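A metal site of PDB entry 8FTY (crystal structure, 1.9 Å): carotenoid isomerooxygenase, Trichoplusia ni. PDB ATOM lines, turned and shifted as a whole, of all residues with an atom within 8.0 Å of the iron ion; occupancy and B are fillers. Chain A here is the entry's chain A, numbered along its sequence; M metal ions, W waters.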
ATOM      1  N   ILE A 138     -18.294 -10.152  35.354  1.00  0.00           N
ATOM      2  CA  ILE A 138     -18.053 -10.259  33.921  1.00  0.00           C
ATOM      3  C   ILE A 138     -16.565 -10.299  33.620  1.00  0.00           C
ATOM      4  O   ILE A 138     -16.107 -11.183  32.903  1.00  0.00           O
ATOM      5  CB  ILE A 138     -18.761  -9.122  33.155  1.00  0.00           C
ATOM      6  CG1 ILE A 138     -20.284  -9.190  33.350  1.00  0.00           C
ATOM      7  CG2 ILE A 138     -18.388  -9.165  31.676  1.00  0.00           C
ATOM      8  CD1 ILE A 138     -21.052  -8.066  32.711  1.00  0.00           C
ATOM      9  N   SER A 139     -15.794  -9.332  34.151  1.00  0.00           N
ATOM     10  CA  SER A 139     -14.428  -9.114  33.702  1.00  0.00           C
ATOM     11  C   SER A 139     -13.549  -8.522  34.789  1.00  0.00           C
ATOM     12  O   SER A 139     -14.041  -8.139  35.851  1.00  0.00           O
ATOM     13  CB  SER A 139     -14.423  -8.224  32.491  1.00  0.00           C
ATOM     14  OG  SER A 139     -14.953  -6.950  32.811  1.00  0.00           O
ATOM     15  N   TYR A 141     -10.024  -5.746  34.745  1.00  0.00           N
ATOM     16  CA  TYR A 141      -9.212  -4.881  33.903  1.00  0.00           C
ATOM     17  C   TYR A 141      -8.213  -4.093  34.744  1.00  0.00           C
ATOM     18  O   TYR A 141      -8.511  -3.695  35.866  1.00  0.00           O
ATOM     19  CB  TYR A 141     -10.100  -3.899  33.117  1.00  0.00           C
ATOM     20  CG  TYR A 141     -10.671  -4.452  31.847  1.00  0.00           C
ATOM     21  CD1 TYR A 141     -11.827  -5.219  31.855  1.00  0.00           C
ATOM     22  CD2 TYR A 141     -10.046  -4.238  30.629  1.00  0.00           C
ATOM     23  CE1 TYR A 141     -12.354  -5.741  30.685  1.00  0.00           C
ATOM     24  CE2 TYR A 141     -10.559  -4.750  29.451  1.00  0.00           C
ATOM     25  CZ  TYR A 141     -11.717  -5.500  29.474  1.00  0.00           C
ATOM     26  OH  TYR A 141     -12.235  -6.012  28.308  1.00  0.00           O
ATOM     27  N   GLU A 152     -21.978  -4.020  34.605  1.00  0.00           N
ATOM     28  CA  GLU A 152     -22.389  -2.903  33.762  1.00  0.00           C
ATOM     29  C   GLU A 152     -23.189  -1.873  34.556  1.00  0.00           C
ATOM     30  O   GLU A 152     -23.453  -0.789  34.057  1.00  0.00           O
ATOM     31  CB  GLU A 152     -23.099  -3.459  32.530  1.00  0.00           C
ATOM     32  CG  GLU A 152     -22.259  -4.509  31.819  1.00  0.00           C
ATOM     33  CD  GLU A 152     -22.560  -4.743  30.350  1.00  0.00           C
ATOM     34  OE1 GLU A 152     -23.730  -4.834  29.997  1.00  0.00           O
ATOM     35  OE2 GLU A 152     -21.585  -4.859  29.577  1.00  0.00           O
ATOM     36  N   SER A 183     -18.650  -3.482  30.379  1.00  0.00           N
ATOM     37  CA  SER A 183     -17.732  -4.259  31.197  1.00  0.00           C
ATOM     38  C   SER A 183     -16.440  -4.542  30.436  1.00  0.00           C
ATOM     39  O   SER A 183     -15.675  -5.414  30.829  1.00  0.00           O
ATOM     40  CB  SER A 183     -18.414  -5.514  31.671  1.00  0.00           C
ATOM     41  OG  SER A 183     -19.096  -6.159  30.598  1.00  0.00           O
ATOM     42  N   HIS A 184     -16.207  -3.779  29.354  1.00  0.00           N
ATOM     43  CA  HIS A 184     -15.060  -3.991  28.486  1.00  0.00           C
ATOM     44  C   HIS A 184     -14.441  -2.647  28.119  1.00  0.00           C
ATOM     45  O   HIS A 184     -14.484  -2.225  26.969  1.00  0.00           O
ATOM     46  CB  HIS A 184     -15.474  -4.780  27.248  1.00  0.00           C
ATOM     47  CG  HIS A 184     -15.793  -6.209  27.538  1.00  0.00           C
ATOM     48  ND1 HIS A 184     -14.835  -7.080  27.998  1.00  0.00           N
ATOM     49  CD2 HIS A 184     -16.925  -6.902  27.451  1.00  0.00           C
ATOM     50  CE1 HIS A 184     -15.386  -8.267  28.190  1.00  0.00           C
ATOM     51  NE2 HIS A 184     -16.656  -8.190  27.864  1.00  0.00           N
ATOM     52  N   TYR A 240     -28.342  -0.663  23.975  1.00  0.00           N
ATOM     53  CA  TYR A 240     -27.448  -1.460  24.798  1.00  0.00           C
ATOM     54  C   TYR A 240     -26.144  -1.728  24.049  1.00  0.00           C
ATOM     55  O   TYR A 240     -26.184  -2.026  22.853  1.00  0.00           O
ATOM     56  CB  TYR A 240     -28.079  -2.797  25.175  1.00  0.00           C
ATOM     57  CG  TYR A 240     -27.120  -3.708  25.892  1.00  0.00           C
ATOM     58  CD1 TYR A 240     -26.724  -3.429  27.195  1.00  0.00           C
ATOM     59  CD2 TYR A 240     -26.526  -4.781  25.246  1.00  0.00           C
ATOM     60  CE1 TYR A 240     -25.809  -4.233  27.852  1.00  0.00           C
ATOM     61  CE2 TYR A 240     -25.607  -5.597  25.897  1.00  0.00           C
ATOM     62  CZ  TYR A 240     -25.245  -5.306  27.201  1.00  0.00           C
ATOM     63  OH  TYR A 240     -24.327  -6.093  27.860  1.00  0.00           O
ATOM     64  N   HIS A 242     -22.297  -3.853  24.851  1.00  0.00           N
ATOM     65  CA  HIS A 242     -21.437  -4.638  25.723  1.00  0.00           C
ATOM     66  C   HIS A 242     -19.980  -4.255  25.488  1.00  0.00           C
ATOM     67  O   HIS A 242     -19.159  -4.354  26.399  1.00  0.00           O
ATOM     68  CB  HIS A 242     -21.693  -6.133  25.505  1.00  0.00           C
ATOM     69  CG  HIS A 242     -20.914  -7.040  26.396  1.00  0.00           C
ATOM     70  ND1 HIS A 242     -21.011  -7.018  27.768  1.00  0.00           N
ATOM     71  CD2 HIS A 242     -20.018  -8.002  26.102  1.00  0.00           C
ATOM     72  CE1 HIS A 242     -20.210  -7.930  28.280  1.00  0.00           C
ATOM     73  NE2 HIS A 242     -19.598  -8.545  27.281  1.00  0.00           N
ATOM     74  N   THR A 243     -19.658  -3.864  24.249  1.00  0.00           N
ATOM     75  CA  THR A 243     -18.319  -3.403  23.895  1.00  0.00           C
ATOM     76  C   THR A 243     -18.426  -2.181  22.998  1.00  0.00           C
ATOM     77  O   THR A 243     -19.503  -1.846  22.502  1.00  0.00           O
ATOM     78  CB  THR A 243     -17.498  -4.517  23.214  1.00  0.00           C
ATOM     79  OG1 THR A 243     -18.241  -5.049  22.105  1.00  0.00           O
ATOM     80  CG2 THR A 243     -17.139  -5.651  24.150  1.00  0.00           C
ATOM     81  N   LEU A 311     -22.109  -8.864  21.091  1.00  0.00           N
ATOM     82  CA  LEU A 311     -21.542  -8.674  22.411  1.00  0.00           C
ATOM     83  C   LEU A 311     -20.130  -8.121  22.269  1.00  0.00           C
ATOM     84  O   LEU A 311     -19.812  -7.080  22.840  1.00  0.00           O
ATOM     85  CB  LEU A 311     -21.538 -10.012  23.154  1.00  0.00           C
ATOM     86  CG  LEU A 311     -22.916 -10.577  23.505  1.00  0.00           C
ATOM     87  CD1 LEU A 311     -22.785 -11.950  24.129  1.00  0.00           C
ATOM     88  CD2 LEU A 311     -23.662  -9.634  24.439  1.00  0.00           C
ATOM     89  N   HIS A 312     -19.290  -8.819  21.491  1.00  0.00           N
ATOM     90  CA  HIS A 312     -17.847  -8.583  21.482  1.00  0.00           C
ATOM     91  C   HIS A 312     -17.368  -8.107  20.109  1.00  0.00           C
ATOM     92  O   HIS A 312     -17.425  -8.850  19.130  1.00  0.00           O
ATOM     93  CB  HIS A 312     -17.101  -9.840  21.942  1.00  0.00           C
ATOM     94  CG  HIS A 312     -17.450 -10.234  23.329  1.00  0.00           C
ATOM     95  ND1 HIS A 312     -18.169 -11.368  23.640  1.00  0.00           N
ATOM     96  CD2 HIS A 312     -17.211  -9.623  24.511  1.00  0.00           C
ATOM     97  CE1 HIS A 312     -18.334 -11.440  24.953  1.00  0.00           C
ATOM     98  NE2 HIS A 312     -17.758 -10.394  25.502  1.00  0.00           N
ATOM     99  N   GLU A 387     -16.798 -16.764  19.755  1.00  0.00           N
ATOM    100  CA  GLU A 387     -17.140 -15.862  20.843  1.00  0.00           C
ATOM    101  C   GLU A 387     -15.945 -15.686  21.775  1.00  0.00           C
ATOM    102  O   GLU A 387     -14.957 -16.405  21.674  1.00  0.00           O
ATOM    103  CB  GLU A 387     -18.363 -16.370  21.627  1.00  0.00           C
ATOM    104  CG  GLU A 387     -19.660 -15.667  21.253  1.00  0.00           C
ATOM    105  CD  GLU A 387     -19.684 -14.171  21.529  1.00  0.00           C
ATOM    106  OE1 GLU A 387     -18.670 -13.628  21.999  1.00  0.00           O
ATOM    107  OE2 GLU A 387     -20.734 -13.543  21.263  1.00  0.00           O
ATOM    108  N   THR A 388     -16.073 -14.693  22.674  1.00  0.00           N
ATOM    109  CA  THR A 388     -15.010 -14.236  23.554  1.00  0.00           C
ATOM    110  C   THR A 388     -13.689 -14.147  22.790  1.00  0.00           C
ATOM    111  O   THR A 388     -12.731 -14.857  23.103  1.00  0.00           O
ATOM    112  CB  THR A 388     -14.912 -15.084  24.821  1.00  0.00           C
ATOM    113  OG1 THR A 388     -14.474 -16.398  24.465  1.00  0.00           O
ATOM    114  CG2 THR A 388     -16.223 -15.152  25.582  1.00  0.00           C
ATOM    115  N   PRO A 389     -13.612 -13.252  21.781  1.00  0.00           N
ATOM    116  CA  PRO A 389     -12.391 -13.101  20.973  1.00  0.00           C
ATOM    117  C   PRO A 389     -11.320 -12.285  21.698  1.00  0.00           C
ATOM    118  O   PRO A 389     -11.643 -11.427  22.512  1.00  0.00           O
ATOM    119  CB  PRO A 389     -12.905 -12.355  19.741  1.00  0.00           C
ATOM    120  CG  PRO A 389     -14.019 -11.484  20.281  1.00  0.00           C
ATOM    121  CD  PRO A 389     -14.682 -12.336  21.347  1.00  0.00           C
ATOM    122  N   GLU A 441     -12.147 -18.395  27.006  1.00  0.00           N
ATOM    123  CA  GLU A 441     -11.508 -17.285  26.330  1.00  0.00           C
ATOM    124  C   GLU A 441      -9.989 -17.450  26.371  1.00  0.00           C
ATOM    125  O   GLU A 441      -9.407 -17.505  27.449  1.00  0.00           O
ATOM    126  CB  GLU A 441     -11.925 -15.990  27.043  1.00  0.00           C
ATOM    127  CG  GLU A 441     -11.192 -14.761  26.558  1.00  0.00           C
ATOM    128  CD  GLU A 441     -11.334 -13.586  27.501  1.00  0.00           C
ATOM    129  OE1 GLU A 441     -10.894 -13.713  28.667  1.00  0.00           O
ATOM    130  OE2 GLU A 441     -11.859 -12.535  27.076  1.00  0.00           O
ATOM    131  N   LEU A 500     -15.754 -16.444  32.593  1.00  0.00           N
ATOM    132  CA  LEU A 500     -16.101 -15.667  31.418  1.00  0.00           C
ATOM    133  C   LEU A 500     -14.858 -14.998  30.821  1.00  0.00           C
ATOM    134  O   LEU A 500     -14.417 -15.376  29.746  1.00  0.00           O
ATOM    135  CB  LEU A 500     -17.145 -14.609  31.779  1.00  0.00           C
ATOM    136  CG  LEU A 500     -18.603 -15.070  31.777  1.00  0.00           C
ATOM    137  CD1 LEU A 500     -19.528 -13.904  32.140  1.00  0.00           C
ATOM    138  CD2 LEU A 500     -18.995 -15.640  30.423  1.00  0.00           C
ATOM    139  N   HIS A 501     -14.334 -13.979  31.516  1.00  0.00           N
ATOM    140  CA  HIS A 501     -13.260 -13.156  30.970  1.00  0.00           C
ATOM    141  C   HIS A 501     -12.122 -13.060  31.984  1.00  0.00           C
ATOM    142  O   HIS A 501     -12.342 -13.218  33.184  1.00  0.00           O
ATOM    143  CB  HIS A 501     -13.747 -11.744  30.651  1.00  0.00           C
ATOM    144  CG  HIS A 501     -14.682 -11.633  29.492  1.00  0.00           C
ATOM    145  ND1 HIS A 501     -14.259 -11.729  28.182  1.00  0.00           N
ATOM    146  CD2 HIS A 501     -15.998 -11.368  29.449  1.00  0.00           C
ATOM    147  CE1 HIS A 501     -15.295 -11.550  27.388  1.00  0.00           C
ATOM    148  NE2 HIS A 501     -16.369 -11.339  28.133  1.00  0.00           N
HETATM  149 FE    FE M   1     -17.954  -9.894  27.514  1.00  0.00          FE
HETATM  150  O   HOH W   1     -19.299 -11.221  28.550  1.00  0.00           O
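OE2 of Glu 441 sits at hydrogen-bond distance from ND1 of His 501, at 2.8 Å. OH of Tyr 141 is in hydrogen-bond range of ND1 of His 184, 2.8 Å away. OE2 of Glu 152 lies within hydrogen-bond range of ND1 of His 242, 2.9 Å away. A ring nitrogen (ND1) of His 312 sits at hydrogen-bond distance from the side-chain carboxylate (OE1) of Glu 387 (2.8 Å). The side-chain hydroxyl of Tyr 240 is in hydrogen-bond range of a ring nitrogen (ND1) of His 242 (3.4 Å).
The iron ion is bound by NE2 of His 312 (2.1 Å), NE2 of His 242 (2.1 Å), water W1 (2.2 Å), NE2 of His 184 (2.2 Å) and NE2 of His 501 (2.2 Å).
Four residues have an atom within 4 Å of the iron ion: His 184, His 242, His 312 and His 501.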
